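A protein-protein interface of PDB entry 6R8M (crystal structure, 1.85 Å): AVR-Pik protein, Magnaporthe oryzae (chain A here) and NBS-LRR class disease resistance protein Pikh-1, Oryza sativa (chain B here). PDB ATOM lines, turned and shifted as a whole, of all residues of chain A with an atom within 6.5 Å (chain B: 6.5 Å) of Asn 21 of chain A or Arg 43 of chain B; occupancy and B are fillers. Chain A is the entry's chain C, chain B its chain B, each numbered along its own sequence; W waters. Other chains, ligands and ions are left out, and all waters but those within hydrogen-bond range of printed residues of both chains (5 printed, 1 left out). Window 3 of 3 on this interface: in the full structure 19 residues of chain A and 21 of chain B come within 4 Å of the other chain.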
ATOM      1  N   ASP A  19       0.337  17.736 -15.962  1.00  0.00           N
ATOM      2  CA  ASP A  19      -0.872  18.566 -16.149  1.00  0.00           C
ATOM      3  C   ASP A  19      -1.737  18.513 -14.882  1.00  0.00           C
ATOM      4  O   ASP A  19      -1.735  17.545 -14.118  1.00  0.00           O
ATOM      5  CB  ASP A  19      -1.713  18.137 -17.354  1.00  0.00           C
ATOM      6  CG  ASP A  19      -1.081  18.339 -18.716  1.00  0.00           C
ATOM      7  OD1 ASP A  19      -0.051  19.004 -18.794  1.00  0.00           O
ATOM      8  OD2 ASP A  19      -1.661  17.821 -19.677  1.00  0.00           O
ATOM      9  N   PRO A  20      -2.518  19.572 -14.622  1.00  0.00           N
ATOM     10  CA  PRO A  20      -3.504  19.544 -13.545  1.00  0.00           C
ATOM     11  C   PRO A  20      -4.610  18.528 -13.838  1.00  0.00           C
ATOM     12  O   PRO A  20      -4.796  18.123 -14.978  1.00  0.00           O
ATOM     13  CB  PRO A  20      -4.138  20.943 -13.522  1.00  0.00           C
ATOM     14  CG  PRO A  20      -3.261  21.771 -14.450  1.00  0.00           C
ATOM     15  CD  PRO A  20      -2.553  20.817 -15.384  1.00  0.00           C
ATOM     16  N   ASN A  21      -5.311  18.172 -12.776  1.00  0.00           N
ATOM     17  CA  ASN A  21      -6.589  17.434 -12.783  1.00  0.00           C
ATOM     18  C   ASN A  21      -7.700  18.483 -12.913  1.00  0.00           C
ATOM     19  O   ASN A  21      -7.873  19.238 -11.968  1.00  0.00           O
ATOM     20  CB  ASN A  21      -6.586  16.512 -11.555  1.00  0.00           C
ATOM     21  CG  ASN A  21      -7.864  15.749 -11.311  1.00  0.00           C
ATOM     22  OD1 ASN A  21      -8.497  15.266 -12.245  1.00  0.00           O
ATOM     23  ND2 ASN A  21      -8.219  15.609 -10.041  1.00  0.00           N
ATOM     24  N   PHE A  22      -8.381  18.518 -14.058  1.00  0.00           N
ATOM     25  CA  PHE A  22      -9.343  19.591 -14.369  1.00  0.00           C
ATOM     26  C   PHE A  22     -10.633  18.984 -14.899  1.00  0.00           C
ATOM     27  O   PHE A  22     -10.691  17.802 -15.287  1.00  0.00           O
ATOM     28  CB  PHE A  22      -8.751  20.566 -15.405  1.00  0.00           C
ATOM     29  CG  PHE A  22      -8.401  19.906 -16.701  1.00  0.00           C
ATOM     30  CD1 PHE A  22      -9.384  19.664 -17.646  1.00  0.00           C
ATOM     31  CD2 PHE A  22      -7.108  19.452 -16.947  1.00  0.00           C
ATOM     32  CE1 PHE A  22      -9.070  19.009 -18.828  1.00  0.00           C
ATOM     33  CE2 PHE A  22      -6.789  18.829 -18.151  1.00  0.00           C
ATOM     34  CZ  PHE A  22      -7.781  18.578 -19.070  1.00  0.00           C
ATOM     35  N   PHE A  23     -11.647  19.801 -14.910  1.00  0.00           N
ATOM     36  CA  PHE A  23     -12.930  19.515 -15.571  1.00  0.00           C
ATOM     37  C   PHE A  23     -13.377  20.758 -16.335  1.00  0.00           C
ATOM     38  O   PHE A  23     -13.646  21.814 -15.720  1.00  0.00           O
ATOM     39  CB  PHE A  23     -13.991  19.056 -14.572  1.00  0.00           C
ATOM     40  CG  PHE A  23     -15.335  18.858 -15.218  1.00  0.00           C
ATOM     41  CD1 PHE A  23     -15.522  17.829 -16.146  1.00  0.00           C
ATOM     42  CD2 PHE A  23     -16.379  19.728 -14.979  1.00  0.00           C
ATOM     43  CE1 PHE A  23     -16.756  17.651 -16.756  1.00  0.00           C
ATOM     44  CE2 PHE A  23     -17.611  19.550 -15.590  1.00  0.00           C
ATOM     45  CZ  PHE A  23     -17.795  18.517 -16.487  1.00  0.00           C
ATOM     46  N   ARG A  43       5.456  22.337  -5.476  1.00  0.00           N
ATOM     47  CA  ARG A  43       4.156  22.476  -6.152  1.00  0.00           C
ATOM     48  C   ARG A  43       3.097  22.226  -5.101  1.00  0.00           C
ATOM     49  O   ARG A  43       3.222  21.208  -4.400  1.00  0.00           O
ATOM     50  CB  ARG A  43       3.988  21.447  -7.263  1.00  0.00           C
ATOM     51  CG  ARG A  43       2.565  21.410  -7.821  1.00  0.00           C
ATOM     52  CD  ARG A  43       2.580  20.570  -9.066  1.00  0.00           C
ATOM     53  NE  ARG A  43       1.274  20.209  -9.614  1.00  0.00           N
ATOM     54  CZ  ARG A  43       1.115  19.782 -10.876  1.00  0.00           C
ATOM     55  NH1 ARG A  43       2.157  19.738 -11.683  1.00  0.00           N
ATOM     56  NH2 ARG A  43      -0.062  19.375 -11.315  1.00  0.00           N
ATOM     57  N   ASP A  45      -0.532  23.021  -5.792  1.00  0.00           N
ATOM     58  CA  ASP A  45      -1.681  22.502  -6.576  1.00  0.00           C
ATOM     59  C   ASP A  45      -1.677  23.198  -7.932  1.00  0.00           C
ATOM     60  O   ASP A  45      -0.762  23.997  -8.195  1.00  0.00           O
ATOM     61  CB  ASP A  45      -3.012  22.723  -5.856  1.00  0.00           C
ATOM     62  CG  ASP A  45      -4.005  21.583  -6.072  1.00  0.00           C
ATOM     63  OD1 ASP A  45      -4.098  21.044  -7.218  1.00  0.00           O
ATOM     64  OD2 ASP A  45      -4.682  21.221  -5.106  1.00  0.00           O
ATOM     65  N   ALA A  46      -2.669  22.899  -8.753  1.00  0.00           N
ATOM     66  CA  ALA A  46      -2.708  23.343 -10.160  1.00  0.00           C
ATOM     67  C   ALA A  46      -4.146  23.280 -10.664  1.00  0.00           C
ATOM     68  O   ALA A  46      -5.007  22.536 -10.081  1.00  0.00           O
ATOM     69  CB  ALA A  46      -1.786  22.469 -10.943  1.00  0.00           C
ATOM     70  N   GLY A  47      -4.432  24.051 -11.708  1.00  0.00           N
ATOM     71  CA  GLY A  47      -5.766  24.033 -12.321  1.00  0.00           C
ATOM     72  C   GLY A  47      -5.752  24.758 -13.651  1.00  0.00           C
ATOM     73  O   GLY A  47      -4.692  24.871 -14.262  1.00  0.00           O
ATOM     74  N   THR A  48      -6.922  25.208 -14.070  1.00  0.00           N
ATOM     75  CA  THR A  48      -7.116  25.920 -15.357  1.00  0.00           C
ATOM     76  C   THR A  48      -7.583  27.346 -15.078  1.00  0.00           C
ATOM     77  O   THR A  48      -8.191  27.641 -14.017  1.00  0.00           O
ATOM     78  CB  THR A  48      -8.087  25.128 -16.226  1.00  0.00           C
ATOM     79  OG1 THR A  48      -9.357  25.170 -15.592  1.00  0.00           O
ATOM     80  CG2 THR A  48      -7.626  23.718 -16.522  1.00  0.00           C
ATOM     81  N   VAL B  12     -12.335  20.663   0.457  1.00  0.00           N
ATOM     82  CA  VAL B  12     -13.118  19.908   1.477  1.00  0.00           C
ATOM     83  C   VAL B  12     -12.173  18.938   2.207  1.00  0.00           C
ATOM     84  O   VAL B  12     -11.407  18.230   1.546  1.00  0.00           O
ATOM     85  CB  VAL B  12     -14.334  19.215   0.826  1.00  0.00           C
ATOM     86  CG1 VAL B  12     -15.297  20.251   0.258  1.00  0.00           C
ATOM     87  CG2 VAL B  12     -13.951  18.230  -0.259  1.00  0.00           C
ATOM     88  N   MET B  14     -11.277  15.390   4.122  1.00  0.00           N
ATOM     89  CA  MET B  14     -11.728  14.031   3.687  1.00  0.00           C
ATOM     90  C   MET B  14     -11.835  13.043   4.866  1.00  0.00           C
ATOM     91  O   MET B  14     -11.025  13.164   5.816  1.00  0.00           O
ATOM     92  CB  MET B  14     -10.781  13.488   2.616  1.00  0.00           C
ATOM     93  CG  MET B  14     -10.775  14.358   1.362  1.00  0.00           C
ATOM     94  SD  MET B  14      -9.761  13.700   0.009  1.00  0.00           S
ATOM     95  CE  MET B  14      -8.096  13.923   0.645  1.00  0.00           C
ATOM     96  N   ARG B  20     -16.245  13.524   0.582  1.00  0.00           N
ATOM     97  CA  ARG B  20     -16.177  14.162  -0.763  1.00  0.00           C
ATOM     98  C   ARG B  20     -17.520  13.926  -1.451  1.00  0.00           C
ATOM     99  O   ARG B  20     -18.045  14.854  -2.039  1.00  0.00           O
ATOM    100  CB  ARG B  20     -14.985  13.648  -1.575  1.00  0.00           C
ATOM    101  CG  ARG B  20     -13.641  14.139  -1.055  1.00  0.00           C
ATOM    102  CD  ARG B  20     -12.538  13.802  -2.039  1.00  0.00           C
ATOM    103  NE  ARG B  20     -12.029  12.440  -1.924  1.00  0.00           N
ATOM    104  CZ  ARG B  20     -11.313  11.807  -2.855  1.00  0.00           C
ATOM    105  NH1 ARG B  20     -11.032  12.390  -4.009  1.00  0.00           N
ATOM    106  NH2 ARG B  20     -10.893  10.571  -2.632  1.00  0.00           N
ATOM    107  N   LEU B  38     -14.764  17.169  -8.966  1.00  0.00           N
ATOM    108  CA  LEU B  38     -13.628  16.892  -8.071  1.00  0.00           C
ATOM    109  C   LEU B  38     -12.383  17.100  -8.888  1.00  0.00           C
ATOM    110  O   LEU B  38     -12.219  16.365  -9.846  1.00  0.00           O
ATOM    111  CB  LEU B  38     -13.696  15.451  -7.567  1.00  0.00           C
ATOM    112  CG  LEU B  38     -14.680  15.254  -6.439  1.00  0.00           C
ATOM    113  CD1 LEU B  38     -14.845  13.774  -6.143  1.00  0.00           C
ATOM    114  CD2 LEU B  38     -14.205  16.019  -5.210  1.00  0.00           C
ATOM    115  N   VAL B  39     -11.601  18.100  -8.511  1.00  0.00           N
ATOM    116  CA  VAL B  39     -10.382  18.503  -9.240  1.00  0.00           C
ATOM    117  C   VAL B  39      -9.248  18.622  -8.225  1.00  0.00           C
ATOM    118  O   VAL B  39      -9.469  18.405  -6.991  1.00  0.00           O
ATOM    119  CB  VAL B  39     -10.631  19.817  -9.996  1.00  0.00           C
ATOM    120  CG1 VAL B  39     -11.728  19.639 -11.043  1.00  0.00           C
ATOM    121  CG2 VAL B  39     -10.969  20.980  -9.093  1.00  0.00           C
ATOM    122  N   GLY B  40      -8.061  18.928  -8.733  1.00  0.00           N
ATOM    123  CA  GLY B  40      -6.895  19.190  -7.864  1.00  0.00           C
ATOM    124  C   GLY B  40      -5.955  18.003  -7.817  1.00  0.00           C
ATOM    125  O   GLY B  40      -6.351  16.864  -8.166  1.00  0.00           O
ATOM    126  N   ASP B  41      -4.707  18.296  -7.464  1.00  0.00           N
ATOM    127  CA  ASP B  41      -3.591  17.336  -7.432  1.00  0.00           C
ATOM    128  C   ASP B  41      -4.004  16.207  -6.477  1.00  0.00           C
ATOM    129  O   ASP B  41      -3.673  15.070  -6.756  1.00  0.00           O
ATOM    130  CB  ASP B  41      -2.293  18.046  -7.029  1.00  0.00           C
ATOM    131  CG  ASP B  41      -1.623  18.825  -8.142  1.00  0.00           C
ATOM    132  OD1 ASP B  41      -2.118  18.729  -9.323  1.00  0.00           O
ATOM    133  OD2 ASP B  41      -0.616  19.553  -7.822  1.00  0.00           O
ATOM    134  N   LEU B  42      -4.788  16.500  -5.450  1.00  0.00           N
ATOM    135  CA  LEU B  42      -5.194  15.491  -4.437  1.00  0.00           C
ATOM    136  C   LEU B  42      -6.688  15.152  -4.550  1.00  0.00           C
ATOM    137  O   LEU B  42      -7.184  14.520  -3.629  1.00  0.00           O
ATOM    138  CB  LEU B  42      -4.860  16.042  -3.050  1.00  0.00           C
ATOM    139  CG  LEU B  42      -3.376  16.262  -2.751  1.00  0.00           C
ATOM    140  CD1 LEU B  42      -3.194  16.958  -1.412  1.00  0.00           C
ATOM    141  CD2 LEU B  42      -2.619  14.947  -2.769  1.00  0.00           C
ATOM    142  N   ARG B  43      -7.401  15.626  -5.577  1.00  0.00           N
ATOM    143  CA  ARG B  43      -8.834  15.326  -5.800  1.00  0.00           C
ATOM    144  C   ARG B  43      -9.639  15.666  -4.543  1.00  0.00           C
ATOM    145  O   ARG B  43     -10.587  14.914  -4.197  1.00  0.00           O
ATOM    146  CB  ARG B  43      -8.948  13.883  -6.309  1.00  0.00           C
ATOM    147  CG  ARG B  43      -8.088  13.624  -7.545  1.00  0.00           C
ATOM    148  CD  ARG B  43      -8.468  12.411  -8.401  1.00  0.00           C
ATOM    149  NE  ARG B  43      -9.918  12.253  -8.529  1.00  0.00           N
ATOM    150  CZ  ARG B  43     -10.683  11.390  -7.841  1.00  0.00           C
ATOM    151  NH1 ARG B  43     -10.151  10.537  -6.978  1.00  0.00           N
ATOM    152  NH2 ARG B  43     -11.991  11.380  -8.031  1.00  0.00           N
ATOM    153  N   ASP B  44      -9.326  16.803  -3.920  1.00  0.00           N
ATOM    154  CA  ASP B  44      -9.940  17.264  -2.651  1.00  0.00           C
ATOM    155  C   ASP B  44     -10.552  18.654  -2.844  1.00  0.00           C
ATOM    156  O   ASP B  44     -10.941  19.280  -1.857  1.00  0.00           O
ATOM    157  CB  ASP B  44      -8.926  17.220  -1.500  1.00  0.00           C
ATOM    158  CG  ASP B  44      -7.731  18.150  -1.654  1.00  0.00           C
ATOM    159  OD1 ASP B  44      -7.495  18.659  -2.768  1.00  0.00           O
ATOM    160  OD2 ASP B  44      -7.012  18.329  -0.659  1.00  0.00           O
ATOM    161  N   LYS B  45     -10.698  19.100  -4.086  1.00  0.00           N
ATOM    162  CA  LYS B  45     -11.294  20.416  -4.395  1.00  0.00           C
ATOM    163  C   LYS B  45     -12.525  20.173  -5.246  1.00  0.00           C
ATOM    164  O   LYS B  45     -12.493  19.307  -6.150  1.00  0.00           O
ATOM    165  CB  LYS B  45     -10.284  21.324  -5.119  1.00  0.00           C
ATOM    166  CG  LYS B  45      -9.076  21.776  -4.303  1.00  0.00           C
ATOM    167  CD  LYS B  45      -8.128  22.689  -5.067  1.00  0.00           C
ATOM    168  CE  LYS B  45      -7.437  22.041  -6.261  1.00  0.00           C
ATOM    169  NZ  LYS B  45      -6.701  23.018  -7.121  1.00  0.00           N
HETATM  170  O   HOH W   1      -7.389  21.540 -10.666  1.00  0.00           O
HETATM  171  O   HOH W   2      -5.923  18.969  -4.608  1.00  0.00           O
HETATM  172  O   HOH W   3      -2.264  16.426 -11.039  1.00  0.00           O
HETATM  173  O   HOH W   4      -9.785  12.354 -11.905  1.00  0.00           O
HETATM  174  O   HOH W   5     -10.862  14.191  -9.912  1.00  0.00           O
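Among the printed residues, merely in contact across the chains: Asn 21 of chain A with Val 39 of chain B (3.4 Å), Asn 21 of chain A with Arg 43 of chain B (3.2 Å), Phe 23 of chain A with Val 39 of chain B (3.9 Å) and Asp 45 of chain A with Gly 40 of chain B (3.4 Å).
Of the printed residues of chain B, Asn 21 of chain A touches Val 39, Gly 40 and Arg 43. Of the printed residues of chain A, Arg 43 of chain B touches Asn 21 (3.2 Å). Of the printed residues of chain A, Lys 45 of chain B touches Asp 45 (3.1 Å) and Ala 46 (3.4 Å). Printed residues of chain B within 4 Å of Arg 43 of chain A: Asp 41 (2.7 Å). Printed residues of chain A within 4 Å of Val 39 of chain B: Asn 21 (3.4 Å) and Phe 23 (3.9 Å).
N of Asp 41 of chain B sits at hydrogen-bond distance from OD1 of Asp 45 of chain A (2.8 Å). OD1 of Asp 45 of chain A lies within salt-bridge range of NZ of Lys 45 of chain B. The guanidinium group of Arg 43 of chain A lies within salt-bridge range of the side-chain carboxylate of Asp 41 of chain B (2.7 Å). The backbone carbonyl oxygen of Ala 46 of chain A sits at hydrogen-bond distance from the side-chain amino group of Lys 45 of chain B (3.4 Å). O of Gly 40 of chain B is in hydrogen-bond range of ND2 of Asn 21 of chain A (2.9 Å).
Of the 10 printed residues of chain A, 5 touch a printed residue of chain B. Of the 11 printed residues of chain B, 5 touch a printed residue of chain A. Hydrophobic or aromatic side chains of chain B that line the printed part of chain A: Val 39. Along chain B the printed residues that touch a printed residue of chain A span positions 39 to 45. Among the printed residues, 9 pairs touch across the chains.
Water W2 lies within hydrogen-bond range of the side-chain carboxylate (OD1) of Asp 44 of chain B, the side-chain carboxylate (OD2) of Asp 45 of chain A, the backbone NH (N) of Leu 42 of chain B and the backbone NH (N) of Asp 41 of chain B. Water W5 lies within hydrogen-bond range of NE of Arg 43 of chain B (2.6 Å), O of Leu 38 of chain B (2.6 Å) and ND2 of Asn 21 of chain A (3.0 Å). Water W1 lies within hydrogen-bond range of O of Ala 46 of chain A (2.6 Å), O of Asn 21 of chain A (2.7 Å) and N of Gly 40 of chain B (3.3 Å). Water W3 bridges OD1 of Asp 41 of chain B (2.9 Å) and O of Asp 19 of chain A (3.3 Å). Water W4 lies within hydrogen-bond range of OD1 of Asn 21 of chain A (3.2 Å) and NE of Arg 43 of chain B (3.4 Å).
The backbone carbonyl oxygen (O) of Arg 43 of chain B sits at hydrogen-bond distance from the guanidinium group (NH1) of Arg 20 of chain B (2.6 Å). The backbone carbonyl oxygen (O) of Val 39 of chain B sits at hydrogen-bond distance from the backbone NH (N) of Asp 44 of chain B, at 3.5 Å. N of Val 39 of chain B is in hydrogen-bond range of O of Lys 45 of chain B, at 2.8 Å.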
